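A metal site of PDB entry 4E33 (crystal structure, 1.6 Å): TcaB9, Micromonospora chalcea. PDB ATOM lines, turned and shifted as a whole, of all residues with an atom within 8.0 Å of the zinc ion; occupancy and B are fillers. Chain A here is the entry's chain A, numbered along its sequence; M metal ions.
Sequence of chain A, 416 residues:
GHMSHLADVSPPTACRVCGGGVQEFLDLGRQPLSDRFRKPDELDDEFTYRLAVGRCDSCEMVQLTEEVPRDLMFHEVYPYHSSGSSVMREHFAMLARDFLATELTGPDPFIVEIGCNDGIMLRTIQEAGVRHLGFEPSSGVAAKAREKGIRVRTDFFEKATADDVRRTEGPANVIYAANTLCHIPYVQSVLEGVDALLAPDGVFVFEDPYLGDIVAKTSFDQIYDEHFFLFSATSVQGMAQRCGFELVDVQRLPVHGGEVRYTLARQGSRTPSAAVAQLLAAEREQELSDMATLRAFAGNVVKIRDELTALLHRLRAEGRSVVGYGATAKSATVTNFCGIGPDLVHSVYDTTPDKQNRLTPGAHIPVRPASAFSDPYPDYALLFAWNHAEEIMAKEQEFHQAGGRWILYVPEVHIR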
ATOM      1  N   ALA A  14      24.718  25.147  10.902  1.00  0.00           N
ATOM      2  CA  ALA A  14      23.863  26.296  11.244  1.00  0.00           C
ATOM      3  C   ALA A  14      23.245  26.146  12.634  1.00  0.00           C
ATOM      4  O   ALA A  14      22.693  25.086  12.955  1.00  0.00           O
ATOM      5  CB  ALA A  14      22.746  26.474  10.221  1.00  0.00           C
ATOM      6  N   CYS A  15      23.299  27.185  13.458  1.00  0.00           N
ATOM      7  CA  CYS A  15      22.634  27.145  14.761  1.00  0.00           C
ATOM      8  C   CYS A  15      21.162  26.760  14.681  1.00  0.00           C
ATOM      9  O   CYS A  15      20.398  27.311  13.889  1.00  0.00           O
ATOM     10  CB  CYS A  15      22.724  28.511  15.441  1.00  0.00           C
ATOM     11  SG  CYS A  15      21.915  28.707  17.056  1.00  0.00           S
ATOM     12  N   ARG A  16      20.763  25.815  15.536  1.00  0.00           N
ATOM     13  CA  ARG A  16      19.383  25.366  15.610  1.00  0.00           C
ATOM     14  C   ARG A  16      18.415  26.344  16.273  1.00  0.00           C
ATOM     15  O   ARG A  16      17.203  26.209  16.151  1.00  0.00           O
ATOM     16  CB  ARG A  16      19.275  23.986  16.267  1.00  0.00           C
ATOM     17  CG  ARG A  16      19.580  22.821  15.359  1.00  0.00           C
ATOM     18  CD  ARG A  16      18.587  22.763  14.157  1.00  0.00           C
ATOM     19  NE  ARG A  16      18.039  21.404  14.059  1.00  0.00           N
ATOM     20  CZ  ARG A  16      16.770  21.063  13.917  1.00  0.00           C
ATOM     21  NH1 ARG A  16      16.498  19.774  13.836  1.00  0.00           N
ATOM     22  NH2 ARG A  16      15.788  21.959  13.827  1.00  0.00           N
ATOM     23  N   VAL A  17      18.962  27.377  16.906  1.00  0.00           N
ATOM     24  CA  VAL A  17      18.115  28.376  17.562  1.00  0.00           C
ATOM     25  C   VAL A  17      17.884  29.502  16.565  1.00  0.00           C
ATOM     26  O   VAL A  17      16.716  29.890  16.384  1.00  0.00           O
ATOM     27  CB  VAL A  17      18.742  28.935  18.860  1.00  0.00           C
ATOM     28  CG1 VAL A  17      18.002  30.178  19.353  1.00  0.00           C
ATOM     29  CG2 VAL A  17      18.663  27.825  19.935  1.00  0.00           C
ATOM     30  N   CYS A  18      18.937  30.019  15.948  1.00  0.00           N
ATOM     31  CA  CYS A  18      18.808  31.282  15.226  1.00  0.00           C
ATOM     32  C   CYS A  18      19.346  31.228  13.806  1.00  0.00           C
ATOM     33  O   CYS A  18      19.216  32.184  13.037  1.00  0.00           O
ATOM     34  CB  CYS A  18      19.447  32.460  15.980  1.00  0.00           C
ATOM     35  SG  CYS A  18      21.251  32.389  15.827  1.00  0.00           S
ATOM     36  N   GLY A  19      19.975  30.130  13.415  1.00  0.00           N
ATOM     37  CA  GLY A  19      20.499  30.022  12.041  1.00  0.00           C
ATOM     38  C   GLY A  19      21.872  30.652  11.887  1.00  0.00           C
ATOM     39  O   GLY A  19      22.418  30.589  10.791  1.00  0.00           O
ATOM     40  N   GLY A  20      22.465  31.209  12.937  1.00  0.00           N
ATOM     41  CA  GLY A  20      23.820  31.772  12.900  1.00  0.00           C
ATOM     42  C   GLY A  20      24.882  30.705  12.686  1.00  0.00           C
ATOM     43  O   GLY A  20      24.591  29.499  12.639  1.00  0.00           O
ATOM     44  N   GLY A  21      26.138  31.114  12.563  1.00  0.00           N
ATOM     45  CA  GLY A  21      27.193  30.143  12.290  1.00  0.00           C
ATOM     46  C   GLY A  21      27.683  29.572  13.605  1.00  0.00           C
ATOM     47  O   GLY A  21      27.799  30.301  14.599  1.00  0.00           O
ATOM     48  N   VAL A  22      27.949  28.264  13.605  1.00  0.00           N
ATOM     49  CA  VAL A  22      28.429  27.602  14.833  1.00  0.00           C
ATOM     50  C   VAL A  22      29.917  27.300  14.693  1.00  0.00           C
ATOM     51  O   VAL A  22      30.313  26.604  13.765  1.00  0.00           O
ATOM     52  CB  VAL A  22      27.688  26.280  15.151  1.00  0.00           C
ATOM     53  CG1 VAL A  22      28.336  25.463  16.278  1.00  0.00           C
ATOM     54  CG2 VAL A  22      26.202  26.587  15.485  1.00  0.00           C
ATOM     55  N   ARG A  55      29.847  26.842  19.416  1.00  0.00           N
ATOM     56  CA  ARG A  55      29.080  27.955  19.981  1.00  0.00           C
ATOM     57  C   ARG A  55      28.556  28.765  18.778  1.00  0.00           C
ATOM     58  O   ARG A  55      29.308  29.121  17.847  1.00  0.00           O
ATOM     59  CB  ARG A  55      29.953  28.812  20.901  1.00  0.00           C
ATOM     60  CG  ARG A  55      29.058  29.830  21.585  1.00  0.00           C
ATOM     61  CD  ARG A  55      29.820  31.082  21.985  1.00  0.00           C
ATOM     62  NE  ARG A  55      30.206  31.829  20.801  1.00  0.00           N
ATOM     63  CZ  ARG A  55      30.937  32.931  20.801  1.00  0.00           C
ATOM     64  NH1 ARG A  55      31.192  33.523  19.620  1.00  0.00           N
ATOM     65  NH2 ARG A  55      31.419  33.416  21.935  1.00  0.00           N
ATOM     66  N   CYS A  56      27.274  29.083  18.787  1.00  0.00           N
ATOM     67  CA  CYS A  56      26.779  29.977  17.739  1.00  0.00           C
ATOM     68  C   CYS A  56      27.426  31.359  17.819  1.00  0.00           C
ATOM     69  O   CYS A  56      27.486  31.930  18.904  1.00  0.00           O
ATOM     70  CB  CYS A  56      25.272  30.166  17.886  1.00  0.00           C
ATOM     71  SG  CYS A  56      24.557  31.289  16.660  1.00  0.00           S
ATOM     72  N   ASP A  57      27.857  31.893  16.688  1.00  0.00           N
ATOM     73  CA  ASP A  57      28.290  33.305  16.601  1.00  0.00           C
ATOM     74  C   ASP A  57      27.283  34.402  16.970  1.00  0.00           C
ATOM     75  O   ASP A  57      27.690  35.484  17.387  1.00  0.00           O
ATOM     76  CB  ASP A  57      28.534  33.662  15.130  1.00  0.00           C
ATOM     77  CG  ASP A  57      29.811  33.073  14.619  1.00  0.00           C
ATOM     78  OD1 ASP A  57      30.640  32.694  15.477  1.00  0.00           O
ATOM     79  OD2 ASP A  57      29.879  33.031  13.372  1.00  0.00           O
ATOM     80  N   SER A  58      26.001  34.148  16.791  1.00  0.00           N
ATOM     81  CA  SER A  58      24.986  35.197  16.898  1.00  0.00           C
ATOM     82  C   SER A  58      24.275  35.146  18.238  1.00  0.00           C
ATOM     83  O   SER A  58      24.145  36.201  18.879  1.00  0.00           O
ATOM     84  CB  SER A  58      24.005  35.074  15.739  1.00  0.00           C
ATOM     85  OG  SER A  58      24.739  35.150  14.528  1.00  0.00           O
ATOM     86  N   CYS A  59      23.829  33.985  18.718  1.00  0.00           N
ATOM     87  CA  CYS A  59      23.078  33.885  19.964  1.00  0.00           C
ATOM     88  C   CYS A  59      23.827  33.264  21.160  1.00  0.00           C
ATOM     89  O   CYS A  59      23.291  33.193  22.275  1.00  0.00           O
ATOM     90  CB  CYS A  59      21.772  33.151  19.706  1.00  0.00           C
ATOM     91  SG  CYS A  59      22.074  31.379  19.578  1.00  0.00           S
ATOM     92  N   GLU A  60      25.054  32.832  20.924  1.00  0.00           N
ATOM     93  CA  GLU A  60      25.892  32.222  21.959  1.00  0.00           C
ATOM     94  C   GLU A  60      25.485  30.845  22.483  1.00  0.00           C
ATOM     95  O   GLU A  60      26.057  30.311  23.448  1.00  0.00           O
ATOM     96  CB  GLU A  60      26.243  33.167  23.124  1.00  0.00           C
ATOM     97  CG  GLU A  60      26.942  34.422  22.577  1.00  0.00           C
ATOM     98  CD  GLU A  60      27.226  35.413  23.708  1.00  0.00           C
ATOM     99  OE1 GLU A  60      28.114  35.127  24.538  1.00  0.00           O
ATOM    100  OE2 GLU A  60      26.560  36.454  23.848  1.00  0.00           O
ATOM    101  N   MET A  61      24.488  30.267  21.817  1.00  0.00           N
ATOM    102  CA  MET A  61      24.075  28.916  22.152  1.00  0.00           C
ATOM    103  C   MET A  61      25.184  27.895  21.833  1.00  0.00           C
ATOM    104  O   MET A  61      25.671  27.720  20.696  1.00  0.00           O
ATOM    105  CB  MET A  61      22.804  28.519  21.421  1.00  0.00           C
ATOM    106  CG  MET A  61      22.304  27.123  21.812  1.00  0.00           C
ATOM    107  SD  MET A  61      21.801  27.059  23.539  1.00  0.00           S
ATOM    108  CE  MET A  61      20.166  27.751  23.464  1.00  0.00           C
ATOM    109  N   VAL A  62      25.580  27.202  22.888  1.00  0.00           N
ATOM    110  CA  VAL A  62      26.529  26.114  22.754  1.00  0.00           C
ATOM    111  C   VAL A  62      25.785  24.821  22.396  1.00  0.00           C
ATOM    112  O   VAL A  62      24.793  24.458  23.037  1.00  0.00           O
ATOM    113  CB  VAL A  62      27.199  25.916  24.127  1.00  0.00           C
ATOM    114  CG1 VAL A  62      28.050  24.663  24.065  1.00  0.00           C
ATOM    115  CG2 VAL A  62      28.093  27.162  24.366  1.00  0.00           C
ATOM    116  N   GLN A  63      26.242  24.092  21.371  1.00  0.00           N
ATOM    117  CA  GLN A  63      25.449  22.967  20.878  1.00  0.00           C
ATOM    118  C   GLN A  63      26.331  21.986  20.110  1.00  0.00           C
ATOM    119  O   GLN A  63      27.377  22.409  19.614  1.00  0.00           O
ATOM    120  CB  GLN A  63      24.342  23.480  19.936  1.00  0.00           C
ATOM    121  CG  GLN A  63      24.861  24.124  18.657  1.00  0.00           C
ATOM    122  CD  GLN A  63      23.828  25.101  18.102  1.00  0.00           C
ATOM    123  OE1 GLN A  63      23.019  24.697  17.268  1.00  0.00           O
ATOM    124  NE2 GLN A  63      23.819  26.348  18.564  1.00  0.00           N
ATOM    125  N   PHE A 229      22.304  20.602  23.514  1.00  0.00           N
ATOM    126  CA  PHE A 229      22.527  21.992  23.931  1.00  0.00           C
ATOM    127  C   PHE A 229      23.130  21.965  25.324  1.00  0.00           C
ATOM    128  O   PHE A 229      22.705  21.205  26.188  1.00  0.00           O
ATOM    129  CB  PHE A 229      21.178  22.724  24.020  1.00  0.00           C
ATOM    130  CG  PHE A 229      20.561  23.012  22.689  1.00  0.00           C
ATOM    131  CD1 PHE A 229      21.176  23.831  21.752  1.00  0.00           C
ATOM    132  CD2 PHE A 229      19.319  22.444  22.383  1.00  0.00           C
ATOM    133  CE1 PHE A 229      20.592  24.067  20.510  1.00  0.00           C
ATOM    134  CE2 PHE A 229      18.706  22.714  21.148  1.00  0.00           C
ATOM    135  CZ  PHE A 229      19.343  23.532  20.222  1.00  0.00           C
ATOM    136  N   SER A 235      22.382  32.284  26.623  1.00  0.00           N
ATOM    137  CA  SER A 235      21.746  31.716  25.440  1.00  0.00           C
ATOM    138  C   SER A 235      20.245  31.503  25.614  1.00  0.00           C
ATOM    139  O   SER A 235      19.469  31.720  24.676  1.00  0.00           O
ATOM    140  CB  SER A 235      22.489  30.436  24.986  1.00  0.00           C
ATOM    141  OG  SER A 235      22.445  29.415  25.987  1.00  0.00           O
ATOM    142  N   MET A 239      17.335  32.822  23.226  1.00  0.00           N
ATOM    143  CA  MET A 239      16.378  31.894  22.645  1.00  0.00           C
ATOM    144  C   MET A 239      14.930  32.238  22.988  1.00  0.00           C
ATOM    145  O   MET A 239      14.036  32.186  22.128  1.00  0.00           O
ATOM    146  CB  MET A 239      16.790  30.516  23.178  1.00  0.00           C
ATOM    147  CG  MET A 239      15.839  29.430  22.682  1.00  0.00           C
ATOM    148  SD  MET A 239      16.214  27.748  23.286  1.00  0.00           S
ATOM    149  CE  MET A 239      15.842  27.853  25.045  1.00  0.00           C
ATOM    150  N   ARG A 242      13.829  35.442  21.124  1.00  0.00           N
ATOM    151  CA  ARG A 242      13.622  35.317  19.683  1.00  0.00           C
ATOM    152  C   ARG A 242      12.290  34.643  19.381  1.00  0.00           C
ATOM    153  O   ARG A 242      11.793  34.777  18.258  1.00  0.00           O
ATOM    154  CB  ARG A 242      14.768  34.582  18.987  1.00  0.00           C
ATOM    155  CG  ARG A 242      16.073  35.362  18.862  1.00  0.00           C
ATOM    156  CD  ARG A 242      17.253  34.397  18.691  1.00  0.00           C
ATOM    157  NE  ARG A 242      18.401  35.058  18.089  1.00  0.00           N
ATOM    158  CZ  ARG A 242      19.425  35.611  18.732  1.00  0.00           C
ATOM    159  NH1 ARG A 242      19.525  35.628  20.061  1.00  0.00           N
ATOM    160  NH2 ARG A 242      20.392  36.166  17.993  1.00  0.00           N
HETATM  161 ZN    ZN M   1      22.282  30.963  17.385  1.00  0.00          ZN
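The side-chain sulfur (SG) of Cys 59 lies close to the backbone NH (N) of Met 61.
The side-chain sulfur (SG) of Cys 15 sits close to the backbone NH (N) of Val 17 (3.2 Å).
The backbone NH (N) of Cys 15 sits at hydrogen-bond distance from the backbone carbonyl oxygen (O) of Gly 20.
NE2 of Gln 63 sits close to SG of Cys 15 (3.4 Å).
SG of Cys 18 lies close to N of Gly 20 (3.3 Å).
The side-chain sulfur of Cys 56 sits close to the backbone NH of Ser 58 (3.2 Å).
N of Cys 56 lies within hydrogen-bond range of O of Met 61 (2.8 Å).
The nearest printed residue that does not touch the zinc ion is Val 17 (4.3 Å).
The zinc ion is bound by the side-chain sulfur (SG) of Cys 59, the side-chain sulfur (SG) of Cys 15, the side-chain sulfur (SG) of Cys 18 and the side-chain sulfur (SG) of Cys 56.
The zinc ion has four donor atoms within binding distance.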
